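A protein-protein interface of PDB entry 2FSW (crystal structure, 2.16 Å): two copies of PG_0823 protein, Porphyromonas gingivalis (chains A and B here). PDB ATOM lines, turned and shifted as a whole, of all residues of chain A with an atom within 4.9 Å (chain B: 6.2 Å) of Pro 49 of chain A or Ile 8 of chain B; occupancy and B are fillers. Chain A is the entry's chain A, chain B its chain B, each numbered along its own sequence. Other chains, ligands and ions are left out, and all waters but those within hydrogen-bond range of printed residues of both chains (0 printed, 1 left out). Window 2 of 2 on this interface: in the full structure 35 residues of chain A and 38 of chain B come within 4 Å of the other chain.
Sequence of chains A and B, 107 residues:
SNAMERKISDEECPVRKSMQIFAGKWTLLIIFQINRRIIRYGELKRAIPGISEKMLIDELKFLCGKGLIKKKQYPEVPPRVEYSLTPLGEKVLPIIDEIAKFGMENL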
ATOM      1  N   GLN A  33       2.622  -7.701  -3.666  1.00  0.00           N
ATOM      2  CA  GLN A  33       2.303  -8.538  -4.836  1.00  0.00           C
ATOM      3  C   GLN A  33       3.469  -8.710  -5.799  1.00  0.00           C
ATOM      4  O   GLN A  33       3.656  -9.795  -6.330  1.00  0.00           O
ATOM      5  CB  GLN A  33       1.054  -8.038  -5.579  1.00  0.00           C
ATOM      6  CG  GLN A  33      -0.261  -8.434  -4.889  1.00  0.00           C
ATOM      7  CD  GLN A  33      -0.500  -9.944  -4.851  1.00  0.00           C
ATOM      8  OE1 GLN A  33      -0.053 -10.684  -5.736  1.00  0.00           O
ATOM      9  NE2 GLN A  33      -1.225 -10.397  -3.844  1.00  0.00           N
ATOM     10  N   LYS A  45      -2.317  -6.036 -12.068  1.00  0.00           N
ATOM     11  CA  LYS A  45      -3.656  -5.455 -12.079  1.00  0.00           C
ATOM     12  C   LYS A  45      -4.693  -6.472 -11.606  1.00  0.00           C
ATOM     13  O   LYS A  45      -5.584  -6.131 -10.828  1.00  0.00           O
ATOM     14  CB  LYS A  45      -3.998  -4.935 -13.483  1.00  0.00           C
ATOM     15  CG  LYS A  45      -4.928  -3.714 -13.539  1.00  0.00           C
ATOM     16  CD  LYS A  45      -6.401  -4.097 -13.619  1.00  0.00           C
ATOM     17  CE  LYS A  45      -7.305  -2.867 -13.718  1.00  0.00           C
ATOM     18  NZ  LYS A  45      -7.686  -2.490 -15.127  1.00  0.00           N
ATOM     19  N   ARG A  46      -4.563  -7.709 -12.083  1.00  0.00           N
ATOM     20  CA  ARG A  46      -5.446  -8.814 -11.701  1.00  0.00           C
ATOM     21  C   ARG A  46      -5.204  -9.304 -10.262  1.00  0.00           C
ATOM     22  O   ARG A  46      -6.133  -9.748  -9.588  1.00  0.00           O
ATOM     23  CB  ARG A  46      -5.318  -9.961 -12.716  1.00  0.00           C
ATOM     24  CG  ARG A  46      -6.479 -10.038 -13.730  1.00  0.00           C
ATOM     25  CD  ARG A  46      -6.036  -9.986 -15.211  1.00  0.00           C
ATOM     26  NE  ARG A  46      -4.995 -11.031 -15.585  1.00  0.00           N
ATOM     27  CZ  ARG A  46      -4.180 -10.788 -16.660  1.00  0.00           C
ATOM     28  NH1 ARG A  46      -4.266  -9.520 -17.502  1.00  0.00           N
ATOM     29  NH2 ARG A  46      -3.262 -11.811 -16.907  1.00  0.00           N
ATOM     30  N   ALA A  47      -3.959  -9.196  -9.798  1.00  0.00           N
ATOM     31  CA  ALA A  47      -3.555  -9.617  -8.440  1.00  0.00           C
ATOM     32  C   ALA A  47      -4.108  -8.727  -7.320  1.00  0.00           C
ATOM     33  O   ALA A  47      -4.095  -9.106  -6.147  1.00  0.00           O
ATOM     34  CB  ALA A  47      -2.041  -9.692  -8.346  1.00  0.00           C
ATOM     35  N   ILE A  48      -4.560  -7.532  -7.686  1.00  0.00           N
ATOM     36  CA  ILE A  48      -5.228  -6.629  -6.745  1.00  0.00           C
ATOM     37  C   ILE A  48      -6.604  -6.222  -7.324  1.00  0.00           C
ATOM     38  O   ILE A  48      -6.745  -5.165  -7.952  1.00  0.00           O
ATOM     39  CB  ILE A  48      -4.345  -5.403  -6.385  1.00  0.00           C
ATOM     40  CG1 ILE A  48      -2.994  -5.860  -5.819  1.00  0.00           C
ATOM     41  CG2 ILE A  48      -5.057  -4.530  -5.361  1.00  0.00           C
ATOM     42  CD1 ILE A  48      -1.794  -5.001  -6.217  1.00  0.00           C
ATOM     43  N   PRO A  49      -7.618  -7.081  -7.127  1.00  0.00           N
ATOM     44  CA  PRO A  49      -8.945  -6.807  -7.683  1.00  0.00           C
ATOM     45  C   PRO A  49      -9.537  -5.502  -7.146  1.00  0.00           C
ATOM     46  O   PRO A  49      -9.430  -5.219  -5.952  1.00  0.00           O
ATOM     47  CB  PRO A  49      -9.783  -8.010  -7.222  1.00  0.00           C
ATOM     48  CG  PRO A  49      -8.794  -9.073  -6.876  1.00  0.00           C
ATOM     49  CD  PRO A  49      -7.577  -8.355  -6.387  1.00  0.00           C
ATOM     50  N   GLY A  50     -10.144  -4.714  -8.032  1.00  0.00           N
ATOM     51  CA  GLY A  50     -10.793  -3.465  -7.637  1.00  0.00           C
ATOM     52  C   GLY A  50      -9.926  -2.220  -7.729  1.00  0.00           C
ATOM     53  O   GLY A  50     -10.368  -1.127  -7.376  1.00  0.00           O
ATOM     54  N   ILE A  51      -8.686  -2.376  -8.185  1.00  0.00           N
ATOM     55  CA  ILE A  51      -7.827  -1.219  -8.421  1.00  0.00           C
ATOM     56  C   ILE A  51      -8.040  -0.733  -9.862  1.00  0.00           C
ATOM     57  O   ILE A  51      -8.065  -1.535 -10.800  1.00  0.00           O
ATOM     58  CB  ILE A  51      -6.317  -1.483  -8.049  1.00  0.00           C
ATOM     59  CG1 ILE A  51      -5.537  -0.164  -7.967  1.00  0.00           C
ATOM     60  CG2 ILE A  51      -5.651  -2.491  -8.995  1.00  0.00           C
ATOM     61  CD1 ILE A  51      -4.108  -0.298  -7.427  1.00  0.00           C
ATOM     62  N   ARG B   6       1.583 -16.289  -7.156  1.00  0.00           N
ATOM     63  CA  ARG B   6       1.364 -16.106  -5.728  1.00  0.00           C
ATOM     64  C   ARG B   6      -0.128 -15.900  -5.507  1.00  0.00           C
ATOM     65  O   ARG B   6      -0.836 -15.507  -6.431  1.00  0.00           O
ATOM     66  CB  ARG B   6       2.153 -14.883  -5.216  1.00  0.00           C
ATOM     67  CG  ARG B   6       3.657 -14.854  -5.610  1.00  0.00           C
ATOM     68  CD  ARG B   6       4.410 -13.655  -5.000  1.00  0.00           C
ATOM     69  NE  ARG B   6       4.288 -13.611  -3.538  1.00  0.00           N
ATOM     70  CZ  ARG B   6       5.120 -14.222  -2.693  1.00  0.00           C
ATOM     71  NH1 ARG B   6       6.154 -14.920  -3.154  1.00  0.00           N
ATOM     72  NH2 ARG B   6       4.919 -14.131  -1.385  1.00  0.00           N
ATOM     73  N   LYS B   7      -0.605 -16.164  -4.291  1.00  0.00           N
ATOM     74  CA  LYS B   7      -1.997 -15.877  -3.919  1.00  0.00           C
ATOM     75  C   LYS B   7      -2.360 -14.424  -4.215  1.00  0.00           C
ATOM     76  O   LYS B   7      -1.558 -13.528  -3.961  1.00  0.00           O
ATOM     77  CB  LYS B   7      -2.204 -16.125  -2.424  1.00  0.00           C
ATOM     78  CG  LYS B   7      -2.640 -17.531  -2.039  1.00  0.00           C
ATOM     79  CD  LYS B   7      -2.892 -17.606  -0.532  1.00  0.00           C
ATOM     80  CE  LYS B   7      -4.072 -16.715  -0.092  1.00  0.00           C
ATOM     81  NZ  LYS B   7      -3.803 -15.958   1.179  1.00  0.00           N
ATOM     82  N   ILE B   8      -3.568 -14.184  -4.732  1.00  0.00           N
ATOM     83  CA  ILE B   8      -3.998 -12.813  -5.026  1.00  0.00           C
ATOM     84  C   ILE B   8      -4.489 -12.088  -3.774  1.00  0.00           C
ATOM     85  O   ILE B   8      -4.844 -12.719  -2.777  1.00  0.00           O
ATOM     86  CB  ILE B   8      -5.060 -12.719  -6.166  1.00  0.00           C
ATOM     87  CG1 ILE B   8      -6.412 -13.283  -5.718  1.00  0.00           C
ATOM     88  CG2 ILE B   8      -4.545 -13.384  -7.459  1.00  0.00           C
ATOM     89  CD1 ILE B   8      -7.596 -12.751  -6.508  1.00  0.00           C
ATOM     90  N   SER B   9      -4.505 -10.759  -3.845  1.00  0.00           N
ATOM     91  CA  SER B   9      -4.980  -9.927  -2.746  1.00  0.00           C
ATOM     92  C   SER B   9      -6.423  -9.475  -2.958  1.00  0.00           C
ATOM     93  O   SER B   9      -6.693  -8.305  -3.244  1.00  0.00           O
ATOM     94  CB  SER B   9      -4.046  -8.728  -2.519  1.00  0.00           C
ATOM     95  OG  SER B   9      -2.798  -9.152  -1.994  1.00  0.00           O
ATOM     96  N   ASP B  10      -7.347 -10.420  -2.816  1.00  0.00           N
ATOM     97  CA  ASP B  10      -8.776 -10.116  -2.842  1.00  0.00           C
ATOM     98  C   ASP B  10      -9.203  -9.509  -1.506  1.00  0.00           C
ATOM     99  O   ASP B  10      -8.361  -9.026  -0.739  1.00  0.00           O
ATOM    100  CB  ASP B  10      -9.594 -11.376  -3.159  1.00  0.00           C
ATOM    101  CG  ASP B  10      -9.157 -12.589  -2.345  1.00  0.00           C
ATOM    102  OD1 ASP B  10      -8.669 -12.426  -1.197  1.00  0.00           O
ATOM    103  OD2 ASP B  10      -9.308 -13.717  -2.864  1.00  0.00           O
ATOM    104  N   GLU B  11     -10.501  -9.541  -1.213  1.00  0.00           N
ATOM    105  CA  GLU B  11     -10.986  -8.986   0.049  1.00  0.00           C
ATOM    106  C   GLU B  11     -10.716  -9.913   1.248  1.00  0.00           C
ATOM    107  O   GLU B  11     -10.983  -9.553   2.394  1.00  0.00           O
ATOM    108  CB  GLU B  11     -12.459  -8.562  -0.040  1.00  0.00           C
ATOM    109  CG  GLU B  11     -12.755  -7.360   0.862  1.00  0.00           C
ATOM    110  CD  GLU B  11     -14.073  -6.653   0.564  1.00  0.00           C
ATOM    111  OE1 GLU B  11     -14.282  -5.558   1.144  1.00  0.00           O
ATOM    112  OE2 GLU B  11     -14.895  -7.179  -0.230  1.00  0.00           O
ATOM    113  N   CYS B  13      -7.449 -11.269   1.575  1.00  0.00           N
ATOM    114  CA  CYS B  13      -6.013 -11.183   1.818  1.00  0.00           C
ATOM    115  C   CYS B  13      -5.705 -10.490   3.161  1.00  0.00           C
ATOM    116  O   CYS B  13      -6.218  -9.398   3.436  1.00  0.00           O
ATOM    117  CB  CYS B  13      -5.288 -10.515   0.641  1.00  0.00           C
ATOM    118  SG  CYS B  13      -3.594  -9.978   0.993  1.00  0.00           S
ATOM    119  N   ARG B  16      -4.377  -6.994   2.712  1.00  0.00           N
ATOM    120  CA  ARG B  16      -5.479  -6.128   2.287  1.00  0.00           C
ATOM    121  C   ARG B  16      -6.492  -5.831   3.399  1.00  0.00           C
ATOM    122  O   ARG B  16      -7.001  -4.706   3.497  1.00  0.00           O
ATOM    123  CB  ARG B  16      -6.180  -6.722   1.054  1.00  0.00           C
ATOM    124  CG  ARG B  16      -7.248  -5.820   0.466  1.00  0.00           C
ATOM    125  CD  ARG B  16      -7.320  -5.955  -1.037  1.00  0.00           C
ATOM    126  NE  ARG B  16      -8.265  -5.000  -1.614  1.00  0.00           N
ATOM    127  CZ  ARG B  16      -8.694  -5.030  -2.874  1.00  0.00           C
ATOM    128  NH1 ARG B  16      -8.275  -5.975  -3.714  1.00  0.00           N
ATOM    129  NH2 ARG B  16      -9.541  -4.107  -3.296  1.00  0.00           N
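Among the printed residues, merely in contact across the chains: Pro 49 of chain A with Ser 9 of chain B (3.3 Å), Gln 33 of chain A with Ile 8 of chain B (3.7 Å), Ala 47 of chain A with Ile 8 of chain B (3.7 Å), Pro 49 of chain A with Ile 8 of chain B (3.9 Å) and Ile 48 of chain A with Arg 16 of chain B (3.9 Å).
The backbone carbonyl oxygen of Lys 7 of chain B sits at hydrogen-bond distance from the side-chain amide nitrogen of Gln 33 of chain A (3.2 Å). The side-chain amide nitrogen (NE2) of Gln 33 of chain A sits at hydrogen-bond distance from the side-chain hydroxyl (OG) of Ser 9 of chain B (2.7 Å). The backbone carbonyl oxygen of Ala 47 of chain A lies within hydrogen-bond range of the backbone NH of Ser 9 of chain B, at 2.9 Å. O of Pro 49 of chain A sits at hydrogen-bond distance from NH1 of Arg 16 of chain B, 2.6 Å away.
Pro 49 of chain A touches just these residues of chain B: Ile 8 (3.9 Å), Ser 9 (3.3 Å) and Arg 16 (2.6 Å). Ile 8 of chain B touches just these residues of chain A: Gln 33, Ala 47 and Pro 49. Printed residues of chain A within 4 Å of Ser 9 of chain B: Gln 33 (2.7 Å), Ala 47 (2.9 Å) and Pro 49 (3.3 Å). Printed residues of chain B within 4 Å of Ala 47 of chain A: Ile 8 and Ser 9. Printed residues of chain B within 4 Å of Ile 48 of chain A: Arg 16 (3.9 Å). Printed residues of chain A within 4 Å of Lys 7 of chain B: Gln 33. Glu 11 of chain B touches none of the printed residues of chain A.
Of the 8 printed residues of chain A, 4 touch a printed residue of chain B. Printed residues of chain A that touch a printed residue of chain B: Gln 33, Ala 47, Ile 48 and Pro 49. Hydrophobic or aromatic side chains of chain A within 4 Å of the printed part of chain B: Ile 48 and Pro 49. Printed residues of chain B that touch a printed residue of chain A: Lys 7, Ile 8, Ser 9 and Arg 16. Hydrophobic or aromatic side chains of chain B that line the printed part of chain A: Ile 8.
No position is printed for both chains. Of the 9 pairs that touch across the chains among the printed residues, none has its exchanged pair printed and touching as well.
OG of Ser 9 of chain B sits at hydrogen-bond distance from SG of Cys 13 of chain B (3.2 Å). The backbone carbonyl oxygen (O) of Ser 9 of chain B lies within hydrogen-bond range of the guanidinium group (NH1) of Arg 16 of chain B, at 2.9 Å. SG of Cys 13 of chain B is in hydrogen-bond range of N of Arg 16 of chain B, at 3.5 Å.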
